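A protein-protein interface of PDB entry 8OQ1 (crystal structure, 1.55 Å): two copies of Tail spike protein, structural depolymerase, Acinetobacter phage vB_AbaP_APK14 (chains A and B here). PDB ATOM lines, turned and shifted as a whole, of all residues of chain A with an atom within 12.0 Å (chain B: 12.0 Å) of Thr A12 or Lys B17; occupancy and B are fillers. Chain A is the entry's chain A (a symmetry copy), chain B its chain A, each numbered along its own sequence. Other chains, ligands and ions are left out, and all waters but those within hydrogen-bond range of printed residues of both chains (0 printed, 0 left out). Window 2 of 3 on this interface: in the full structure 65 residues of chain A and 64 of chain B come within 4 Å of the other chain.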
ATOM      1  N   THR A  12      -8.398  -1.203 -22.186  1.00  0.00           N
ATOM      2  CA  THR A  12      -7.012  -0.632 -22.136  1.00  0.00           C
ATOM      3  C   THR A  12      -5.969  -1.760 -22.047  1.00  0.00           C
ATOM      4  O   THR A  12      -5.419  -1.947 -20.966  1.00  0.00           O
ATOM      5  CB  THR A  12      -6.906   0.429 -21.021  1.00  0.00           C
ATOM      6  OG1 THR A  12      -5.515   0.718 -20.855  1.00  0.00           O
ATOM      7  CG2 THR A  12      -7.555   0.036 -19.702  1.00  0.00           C
ATOM      8  N   ARG A  13      -5.687  -2.453 -23.156  1.00  0.00           N
ATOM      9  CA  ARG A  13      -4.800  -3.654 -23.215  1.00  0.00           C
ATOM     10  C   ARG A  13      -3.340  -3.226 -23.465  1.00  0.00           C
ATOM     11  O   ARG A  13      -3.111  -2.194 -24.138  1.00  0.00           O
ATOM     12  CB  ARG A  13      -5.268  -4.652 -24.284  1.00  0.00           C
ATOM     13  N   SER A  14      -2.409  -3.984 -22.870  1.00  0.00           N
ATOM     14  CA  SER A  14      -0.934  -4.014 -23.078  1.00  0.00           C
ATOM     15  C   SER A  14      -0.586  -4.109 -24.574  1.00  0.00           C
ATOM     16  O   SER A  14      -1.261  -4.878 -25.310  1.00  0.00           O
ATOM     17  CB  SER A  14      -0.346  -5.182 -22.300  1.00  0.00           C
ATOM     18  OG  SER A  14       0.977  -5.476 -22.715  1.00  0.00           O
ATOM     19  N   ALA A  15       0.462  -3.390 -25.012  1.00  0.00           N
ATOM     20  CA  ALA A  15       1.021  -3.471 -26.386  1.00  0.00           C
ATOM     21  C   ALA A  15       1.612  -4.866 -26.619  1.00  0.00           C
ATOM     22  O   ALA A  15       1.455  -5.367 -27.772  1.00  0.00           O
ATOM     23  CB  ALA A  15       2.042  -2.379 -26.602  1.00  0.00           C
ATOM     24  N   ASP A  16       2.208  -5.461 -25.562  1.00  0.00           N
ATOM     25  CA  ASP A  16       2.576  -6.904 -25.386  1.00  0.00           C
ATOM     26  C   ASP A  16       1.436  -7.865 -25.821  1.00  0.00           C
ATOM     27  O   ASP A  16       1.766  -8.984 -26.336  1.00  0.00           O
ATOM     28  CB  ASP A  16       3.055  -7.162 -23.942  1.00  0.00           C
ATOM     29  N   LYS A  17       0.153  -7.473 -25.670  1.00  0.00           N
ATOM     30  CA  LYS A  17      -1.058  -8.300 -25.977  1.00  0.00           C
ATOM     31  C   LYS A  17      -1.540  -8.103 -27.432  1.00  0.00           C
ATOM     32  O   LYS A  17      -2.396  -8.911 -27.870  1.00  0.00           O
ATOM     33  CB  LYS A  17      -2.181  -8.017 -24.967  1.00  0.00           C
ATOM     34  N   VAL A  18      -1.033  -7.119 -28.192  1.00  0.00           N
ATOM     35  CA  VAL A  18      -1.431  -6.894 -29.618  1.00  0.00           C
ATOM     36  C   VAL A  18      -0.421  -7.627 -30.506  1.00  0.00           C
ATOM     37  O   VAL A  18       0.781  -7.449 -30.226  1.00  0.00           O
ATOM     38  CB  VAL A  18      -1.495  -5.394 -29.955  1.00  0.00           C
ATOM     39  CG1 VAL A  18      -2.096  -5.152 -31.333  1.00  0.00           C
ATOM     40  CG2 VAL A  18      -2.219  -4.583 -28.888  1.00  0.00           C
ATOM     41  N   GLN A  26       2.995  -5.873 -30.783  1.00  0.00           N
ATOM     42  CA  GLN A  26       3.124  -4.408 -30.945  1.00  0.00           C
ATOM     43  C   GLN A  26       4.272  -3.895 -30.086  1.00  0.00           C
ATOM     44  O   GLN A  26       5.005  -3.060 -30.613  1.00  0.00           O
ATOM     45  CB  GLN A  26       1.848  -3.623 -30.635  1.00  0.00           C
ATOM     46  CG  GLN A  26       1.831  -2.242 -31.274  1.00  0.00           C
ATOM     47  CD  GLN A  26       2.134  -2.312 -32.740  1.00  0.00           C
ATOM     48  OE1 GLN A  26       3.035  -1.635 -33.241  1.00  0.00           O
ATOM     49  NE2 GLN A  26       1.521  -3.264 -33.409  1.00  0.00           N
ATOM     50  N   GLN A  27       4.486  -4.421 -28.875  1.00  0.00           N
ATOM     51  CA  GLN A  27       5.594  -3.998 -27.997  1.00  0.00           C
ATOM     52  C   GLN A  27       6.941  -4.305 -28.669  1.00  0.00           C
ATOM     53  O   GLN A  27       7.790  -3.371 -28.676  1.00  0.00           O
ATOM     54  CB  GLN A  27       5.497  -4.629 -26.605  1.00  0.00           C
ATOM     55  CG  GLN A  27       6.527  -4.104 -25.612  1.00  0.00           C
ATOM     56  CD  GLN A  27       6.336  -2.631 -25.377  1.00  0.00           C
ATOM     57  OE1 GLN A  27       5.275  -2.183 -24.945  1.00  0.00           O
ATOM     58  NE2 GLN A  27       7.335  -1.856 -25.757  1.00  0.00           N
ATOM     59  N   ASN A  30       7.292  -1.813 -31.533  1.00  0.00           N
ATOM     60  CA  ASN A  30       7.531  -0.438 -31.006  1.00  0.00           C
ATOM     61  C   ASN A  30       8.987  -0.272 -30.574  1.00  0.00           C
ATOM     62  O   ASN A  30       9.542   0.785 -30.836  1.00  0.00           O
ATOM     63  CB  ASN A  30       6.657  -0.035 -29.812  1.00  0.00           C
ATOM     64  CG  ASN A  30       5.173  -0.093 -30.101  1.00  0.00           C
ATOM     65  OD1 ASN A  30       4.743  -0.160 -31.258  1.00  0.00           O
ATOM     66  ND2 ASN A  30       4.394  -0.141 -29.032  1.00  0.00           N
ATOM     67  N   THR B  12     -12.584  -4.250 -31.798  1.00  0.00           N
ATOM     68  CA  THR B  12     -12.007  -3.146 -32.634  1.00  0.00           C
ATOM     69  C   THR B  12     -11.732  -1.904 -31.767  1.00  0.00           C
ATOM     70  O   THR B  12     -12.494  -0.948 -31.878  1.00  0.00           O
ATOM     71  CB  THR B  12     -12.896  -2.883 -33.867  1.00  0.00           C
ATOM     72  OG1 THR B  12     -12.444  -1.658 -34.450  1.00  0.00           O
ATOM     73  CG2 THR B  12     -14.390  -2.844 -33.581  1.00  0.00           C
ATOM     74  N   ARG B  13     -10.660  -1.914 -30.967  1.00  0.00           N
ATOM     75  CA  ARG B  13     -10.321  -0.850 -29.974  1.00  0.00           C
ATOM     76  C   ARG B  13      -9.452   0.239 -30.636  1.00  0.00           C
ATOM     77  O   ARG B  13      -8.673  -0.080 -31.564  1.00  0.00           O
ATOM     78  CB  ARG B  13      -9.621  -1.432 -28.737  1.00  0.00           C
ATOM     79  N   SER B  14      -9.654   1.486 -30.189  1.00  0.00           N
ATOM     80  CA  SER B  14      -8.850   2.718 -30.419  1.00  0.00           C
ATOM     81  C   SER B  14      -7.357   2.467 -30.144  1.00  0.00           C
ATOM     82  O   SER B  14      -7.028   1.774 -29.143  1.00  0.00           O
ATOM     83  CB  SER B  14      -9.391   3.836 -29.539  1.00  0.00           C
ATOM     84  OG  SER B  14      -8.483   4.919 -29.449  1.00  0.00           O
ATOM     85  N   ALA B  15      -6.470   3.044 -30.972  1.00  0.00           N
ATOM     86  CA  ALA B  15      -4.998   3.024 -30.774  1.00  0.00           C
ATOM     87  C   ALA B  15      -4.639   3.806 -29.505  1.00  0.00           C
ATOM     88  O   ALA B  15      -3.697   3.343 -28.796  1.00  0.00           O
ATOM     89  CB  ALA B  15      -4.296   3.570 -31.996  1.00  0.00           C
ATOM     90  N   ASP B  16      -5.390   4.895 -29.229  1.00  0.00           N
ATOM     91  CA  ASP B  16      -5.497   5.652 -27.938  1.00  0.00           C
ATOM     92  C   ASP B  16      -5.650   4.713 -26.710  1.00  0.00           C
ATOM     93  O   ASP B  16      -5.126   5.084 -25.608  1.00  0.00           O
ATOM     94  CB  ASP B  16      -6.622   6.705 -28.027  1.00  0.00           C
ATOM     95  N   LYS B  17      -6.296   3.537 -26.859  1.00  0.00           N
ATOM     96  CA  LYS B  17      -6.585   2.552 -25.767  1.00  0.00           C
ATOM     97  C   LYS B  17      -5.456   1.507 -25.616  1.00  0.00           C
ATOM     98  O   LYS B  17      -5.476   0.780 -24.593  1.00  0.00           O
ATOM     99  CB  LYS B  17      -7.949   1.880 -25.988  1.00  0.00           C
ATOM    100  N   VAL B  18      -4.485   1.414 -26.540  1.00  0.00           N
ATOM    101  CA  VAL B  18      -3.345   0.447 -26.437  1.00  0.00           C
ATOM    102  C   VAL B  18      -2.170   1.180 -25.782  1.00  0.00           C
ATOM    103  O   VAL B  18      -1.908   2.309 -26.239  1.00  0.00           O
ATOM    104  CB  VAL B  18      -2.960  -0.116 -27.816  1.00  0.00           C
ATOM    105  CG1 VAL B  18      -1.947  -1.248 -27.698  1.00  0.00           C
ATOM    106  CG2 VAL B  18      -4.170  -0.545 -28.635  1.00  0.00           C
ATOM    107  N   ILE B  19      -1.466   0.545 -24.823  1.00  0.00           N
ATOM    108  CA  ILE B  19      -0.461   1.181 -23.900  1.00  0.00           C
ATOM    109  C   ILE B  19       0.874   0.419 -23.966  1.00  0.00           C
ATOM    110  O   ILE B  19       0.861  -0.833 -23.904  1.00  0.00           O
ATOM    111  CB  ILE B  19      -0.948   1.270 -22.430  1.00  0.00           C
ATOM    112  CG1 ILE B  19      -2.416   1.677 -22.287  1.00  0.00           C
ATOM    113  CG2 ILE B  19      -0.048   2.196 -21.613  1.00  0.00           C
ATOM    114  CD1 ILE B  19      -2.745   3.062 -22.792  1.00  0.00           C
ATOM    115  N   ASP B  20       1.978   1.178 -23.990  1.00  0.00           N
ATOM    116  CA  ASP B  20       3.376   0.722 -24.224  1.00  0.00           C
ATOM    117  C   ASP B  20       4.081   0.539 -22.873  1.00  0.00           C
ATOM    118  O   ASP B  20       3.806   1.334 -21.981  1.00  0.00           O
ATOM    119  CB  ASP B  20       4.105   1.760 -25.097  1.00  0.00           C
ATOM    120  CG  ASP B  20       5.493   1.369 -25.586  1.00  0.00           C
ATOM    121  OD1 ASP B  20       5.583   0.681 -26.612  1.00  0.00           O
ATOM    122  OD2 ASP B  20       6.471   1.772 -24.951  1.00  0.00           O
ATOM    123  N   GLU B  21       5.044  -0.394 -22.778  1.00  0.00           N
ATOM    124  CA  GLU B  21       6.010  -0.587 -21.652  1.00  0.00           C
ATOM    125  C   GLU B  21       6.695   0.731 -21.216  1.00  0.00           C
ATOM    126  O   GLU B  21       7.433   0.668 -20.206  1.00  0.00           O
ATOM    127  CB  GLU B  21       7.086  -1.619 -22.027  1.00  0.00           C
ATOM    128  N   SER B  22       6.517   1.850 -21.953  1.00  0.00           N
ATOM    129  CA  SER B  22       6.907   3.247 -21.597  1.00  0.00           C
ATOM    130  C   SER B  22       5.774   4.026 -20.929  1.00  0.00           C
ATOM    131  O   SER B  22       6.043   5.160 -20.547  1.00  0.00           O
ATOM    132  CB  SER B  22       7.320   4.009 -22.830  1.00  0.00           C
ATOM    133  OG  SER B  22       6.174   4.259 -23.646  1.00  0.00           O
ATOM    134  N   GLY B  23       4.560   3.475 -20.876  1.00  0.00           N
ATOM    135  CA  GLY B  23       3.296   4.203 -20.653  1.00  0.00           C
ATOM    136  C   GLY B  23       3.036   5.309 -21.671  1.00  0.00           C
ATOM    137  O   GLY B  23       3.065   6.489 -21.275  1.00  0.00           O
ATOM    138  N   ALA B  24       2.779   4.968 -22.936  1.00  0.00           N
ATOM    139  CA  ALA B  24       2.322   5.913 -23.986  1.00  0.00           C
ATOM    140  C   ALA B  24       1.338   5.175 -24.871  1.00  0.00           C
ATOM    141  O   ALA B  24       1.516   3.952 -25.043  1.00  0.00           O
ATOM    142  CB  ALA B  24       3.521   6.433 -24.775  1.00  0.00           C
ATOM    143  N   THR B  25       0.372   5.892 -25.434  1.00  0.00           N
ATOM    144  CA  THR B  25      -0.659   5.284 -26.304  1.00  0.00           C
ATOM    145  C   THR B  25       0.056   4.792 -27.561  1.00  0.00           C
ATOM    146  O   THR B  25       0.969   5.480 -28.008  1.00  0.00           O
ATOM    147  CB  THR B  25      -1.824   6.235 -26.604  1.00  0.00           C
ATOM    148  OG1 THR B  25      -1.343   7.287 -27.428  1.00  0.00           O
ATOM    149  CG2 THR B  25      -2.461   6.826 -25.358  1.00  0.00           C
ATOM    150  N   GLN B  26      -0.362   3.658 -28.107  1.00  0.00           N
ATOM    151  CA  GLN B  26      -0.057   3.342 -29.520  1.00  0.00           C
ATOM    152  C   GLN B  26      -0.317   4.565 -30.389  1.00  0.00           C
ATOM    153  O   GLN B  26       0.527   4.800 -31.251  1.00  0.00           O
ATOM    154  CB  GLN B  26      -0.817   2.136 -30.077  1.00  0.00           C
ATOM    155  CG  GLN B  26      -0.146   1.524 -31.299  1.00  0.00           C
ATOM    156  CD  GLN B  26       1.303   1.239 -31.044  1.00  0.00           C
ATOM    157  OE1 GLN B  26       2.182   1.672 -31.793  1.00  0.00           O
ATOM    158  NE2 GLN B  26       1.584   0.673 -29.890  1.00  0.00           N
ATOM    159  N   GLN B  27      -1.361   5.360 -30.127  1.00  0.00           N
ATOM    160  CA  GLN B  27      -1.661   6.578 -30.904  1.00  0.00           C
ATOM    161  C   GLN B  27      -0.510   7.586 -30.762  1.00  0.00           C
ATOM    162  O   GLN B  27      -0.082   8.102 -31.832  1.00  0.00           O
ATOM    163  CB  GLN B  27      -3.007   7.193 -30.510  1.00  0.00           C
ATOM    164  CG  GLN B  27      -3.437   8.362 -31.389  1.00  0.00           C
ATOM    165  CD  GLN B  27      -3.624   7.915 -32.813  1.00  0.00           C
ATOM    166  OE1 GLN B  27      -4.427   7.032 -33.106  1.00  0.00           O
ATOM    167  NE2 GLN B  27      -2.806   8.459 -33.695  1.00  0.00           N
ATOM    168  N   GLU B  28      -0.001   7.833 -29.538  1.00  0.00           N
ATOM    169  CA  GLU B  28       1.109   8.803 -29.319  1.00  0.00           C
ATOM    170  C   GLU B  28       2.345   8.283 -30.073  1.00  0.00           C
ATOM    171  O   GLU B  28       3.000   9.097 -30.717  1.00  0.00           O
ATOM    172  CB  GLU B  28       1.411   9.058 -27.837  1.00  0.00           C
ATOM    173  N   LEU B  29       2.635   6.971 -29.999  1.00  0.00           N
ATOM    174  CA  LEU B  29       3.769   6.324 -30.715  1.00  0.00           C
ATOM    175  C   LEU B  29       3.598   6.451 -32.229  1.00  0.00           C
ATOM    176  O   LEU B  29       4.592   6.858 -32.916  1.00  0.00           O
ATOM    177  CB  LEU B  29       3.880   4.853 -30.324  1.00  0.00           C
ATOM    178  CG  LEU B  29       4.528   4.562 -28.984  1.00  0.00           C
ATOM    179  CD1 LEU B  29       4.423   3.078 -28.694  1.00  0.00           C
ATOM    180  CD2 LEU B  29       5.991   4.964 -28.975  1.00  0.00           C
ATOM    181  N   ASN B  30       2.407   6.154 -32.755  1.00  0.00           N
ATOM    182  CA  ASN B  30       2.129   6.227 -34.219  1.00  0.00           C
ATOM    183  C   ASN B  30       2.360   7.644 -34.741  1.00  0.00           C
ATOM    184  O   ASN B  30       2.905   7.769 -35.829  1.00  0.00           O
ATOM    185  CB  ASN B  30       0.711   5.819 -34.635  1.00  0.00           C
ATOM    186  CG  ASN B  30       0.346   4.405 -34.236  1.00  0.00           C
ATOM    187  OD1 ASN B  30       1.209   3.590 -33.890  1.00  0.00           O
ATOM    188  ND2 ASN B  30      -0.951   4.144 -34.214  1.00  0.00           N
ATOM    189  N   ASN B  31       2.028   8.672 -33.972  1.00  0.00           N
ATOM    190  CA  ASN B  31       2.277  10.077 -34.386  1.00  0.00           C
ATOM    191  C   ASN B  31       3.786  10.353 -34.477  1.00  0.00           C
ATOM    192  O   ASN B  31       4.145  11.355 -35.141  1.00  0.00           O
ATOM    193  CB  ASN B  31       1.629  11.078 -33.420  1.00  0.00           C
ATOM    194  CG  ASN B  31       0.147  10.836 -33.198  1.00  0.00           C
ATOM    195  OD1 ASN B  31      -0.331  10.985 -32.070  1.00  0.00           O
ATOM    196  ND2 ASN B  31      -0.576  10.456 -34.249  1.00  0.00           N
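Of the 20 printed residues of chain B, 7 touch a printed residue of chain A.
Printed residues of chain B that touch a printed residue of chain A: Lys B17, Val B18, Ile B19, Asp B20, Glu B21, Gln B26 and Leu B29.
Of the 10 printed residues of chain A, 8 touch a printed residue of chain B.
Printed residues of chain A that touch a printed residue of chain B: Thr A12, Arg A13, Ser A14, Ala A15, Val A18, Gln A26, Gln A27 and Asn A30.
Hydrophobic or aromatic side chains of chain A within 4 Å of the printed part of chain B: Ala A15 and Val A18.
Among the printed residues, no Asp or Glu carboxylate lies within 4 Å of a Lys or Arg side-chain nitrogen of the other chain.
O of Arg A13 lies within hydrogen-bond range of N of Ile B19 (3.3 Å).
N of Ala A15 is in hydrogen-bond range of O of Ile B19 (2.8 Å).
The side-chain carboxylate (OD1) of Asp B20 lies within hydrogen-bond range of the side-chain amide nitrogen (NE2) of Gln A27 (3.2 Å).
The side-chain carboxylate (OD1) of Asp B20 sits at hydrogen-bond distance from the side-chain amide nitrogen (ND2) of Asn A30 (2.8 Å).
OE1 of Gln A27 is in hydrogen-bond range of N of Glu B21, 2.8 Å away.
The side-chain amide nitrogen (NE2) of Gln B26 sits close to the side-chain amide nitrogen (ND2) of Asn A30 (3.0 Å).
Thr A12 touches Lys B17, but with the chains exchanged Lys A17 does not touch Thr B12 (11.9 Å).
Arg A13 touches Val B18, but with the chains exchanged Val A18 does not touch Arg B13 (8.0 Å).
Val B18 touches its own counterpart, Val A18.
Gln B26 touches its own counterpart, Gln A26.
Of the 15 pairs that touch across the chains among the printed residues, 2 have their exchanged pair printed and touching as well.
Lys B17 touches Thr A12 (O to CA, 3.2 Å).
CG1 of Ile B19 touches OG1 of Thr A12 (3.5 Å).
O of Lys B17 touches N of Arg A13, at 3.5 Å.
Arg A13 touches Val B18.
O of Ile B19 touches C of Ser A14, at 3.6 Å.
CA of Ala A15 touches CG1 of Val B18 (3.9 Å).
Val A18 touches Val B18 (CG2 to CG1, 3.6 Å).
Gln B26 touches Gln A26.
Leu B29 touches Asn A30 (CD1 to ND2, 3.2 Å).
N of Gln B26 sits close to O of Ala B15 (3.4 Å).
The side-chain hydroxyl (OG) of Ser B22 sits at hydrogen-bond distance from the side-chain carboxylate (OD2) of Asp B20.
The backbone carbonyl oxygen (O) of Gln B26 sits close to the side-chain amide oxygen (OD1) of Asn B30 (3.0 Å).
The backbone carbonyl oxygen (O) of Ala A15 sits at hydrogen-bond distance from the backbone NH (N) of Gln A27 (3.4 Å).
The backbone NH of Gln A26 sits at hydrogen-bond distance from the backbone carbonyl oxygen of Val A18 (2.8 Å).
O of Gln A26 lies close to OD1 of Asn A30.
Of chain B, only Lys B17 (3.2 Å) and Ile B19 (3.5 Å) come within 4 Å of Thr A12.
Printed residues of chain B within 4 Å of Arg A13: Lys B17, Val B18 and Ile B19.
Of the printed residues of chain B, Val A18 touches Val B18.
No residue of chain A comes within 4 Å of Arg B13.
No residue of chain A comes within 4 Å of Ser B14.
No residue of chain A comes within 4 Å of Ala B15.
No residue of chain A comes within 4 Å of Asp B16.
Val B18 touches just these residues of chain A: Arg A13 (3.5 Å), Ala A15 (3.9 Å) and Val A18 (3.6 Å).
Of chain A, only Thr A12 (3.5 Å), Arg A13 (3.3 Å), Ser A14 (3.6 Å) and Ala A15 (2.8 Å) come within 4 Å of Ile B19.
Of the printed residues of chain A, Asp B20 touches Gln A27 (3.2 Å) and Asn A30 (2.8 Å).
Of the printed residues of chain A, Leu B29 touches Asn A30.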
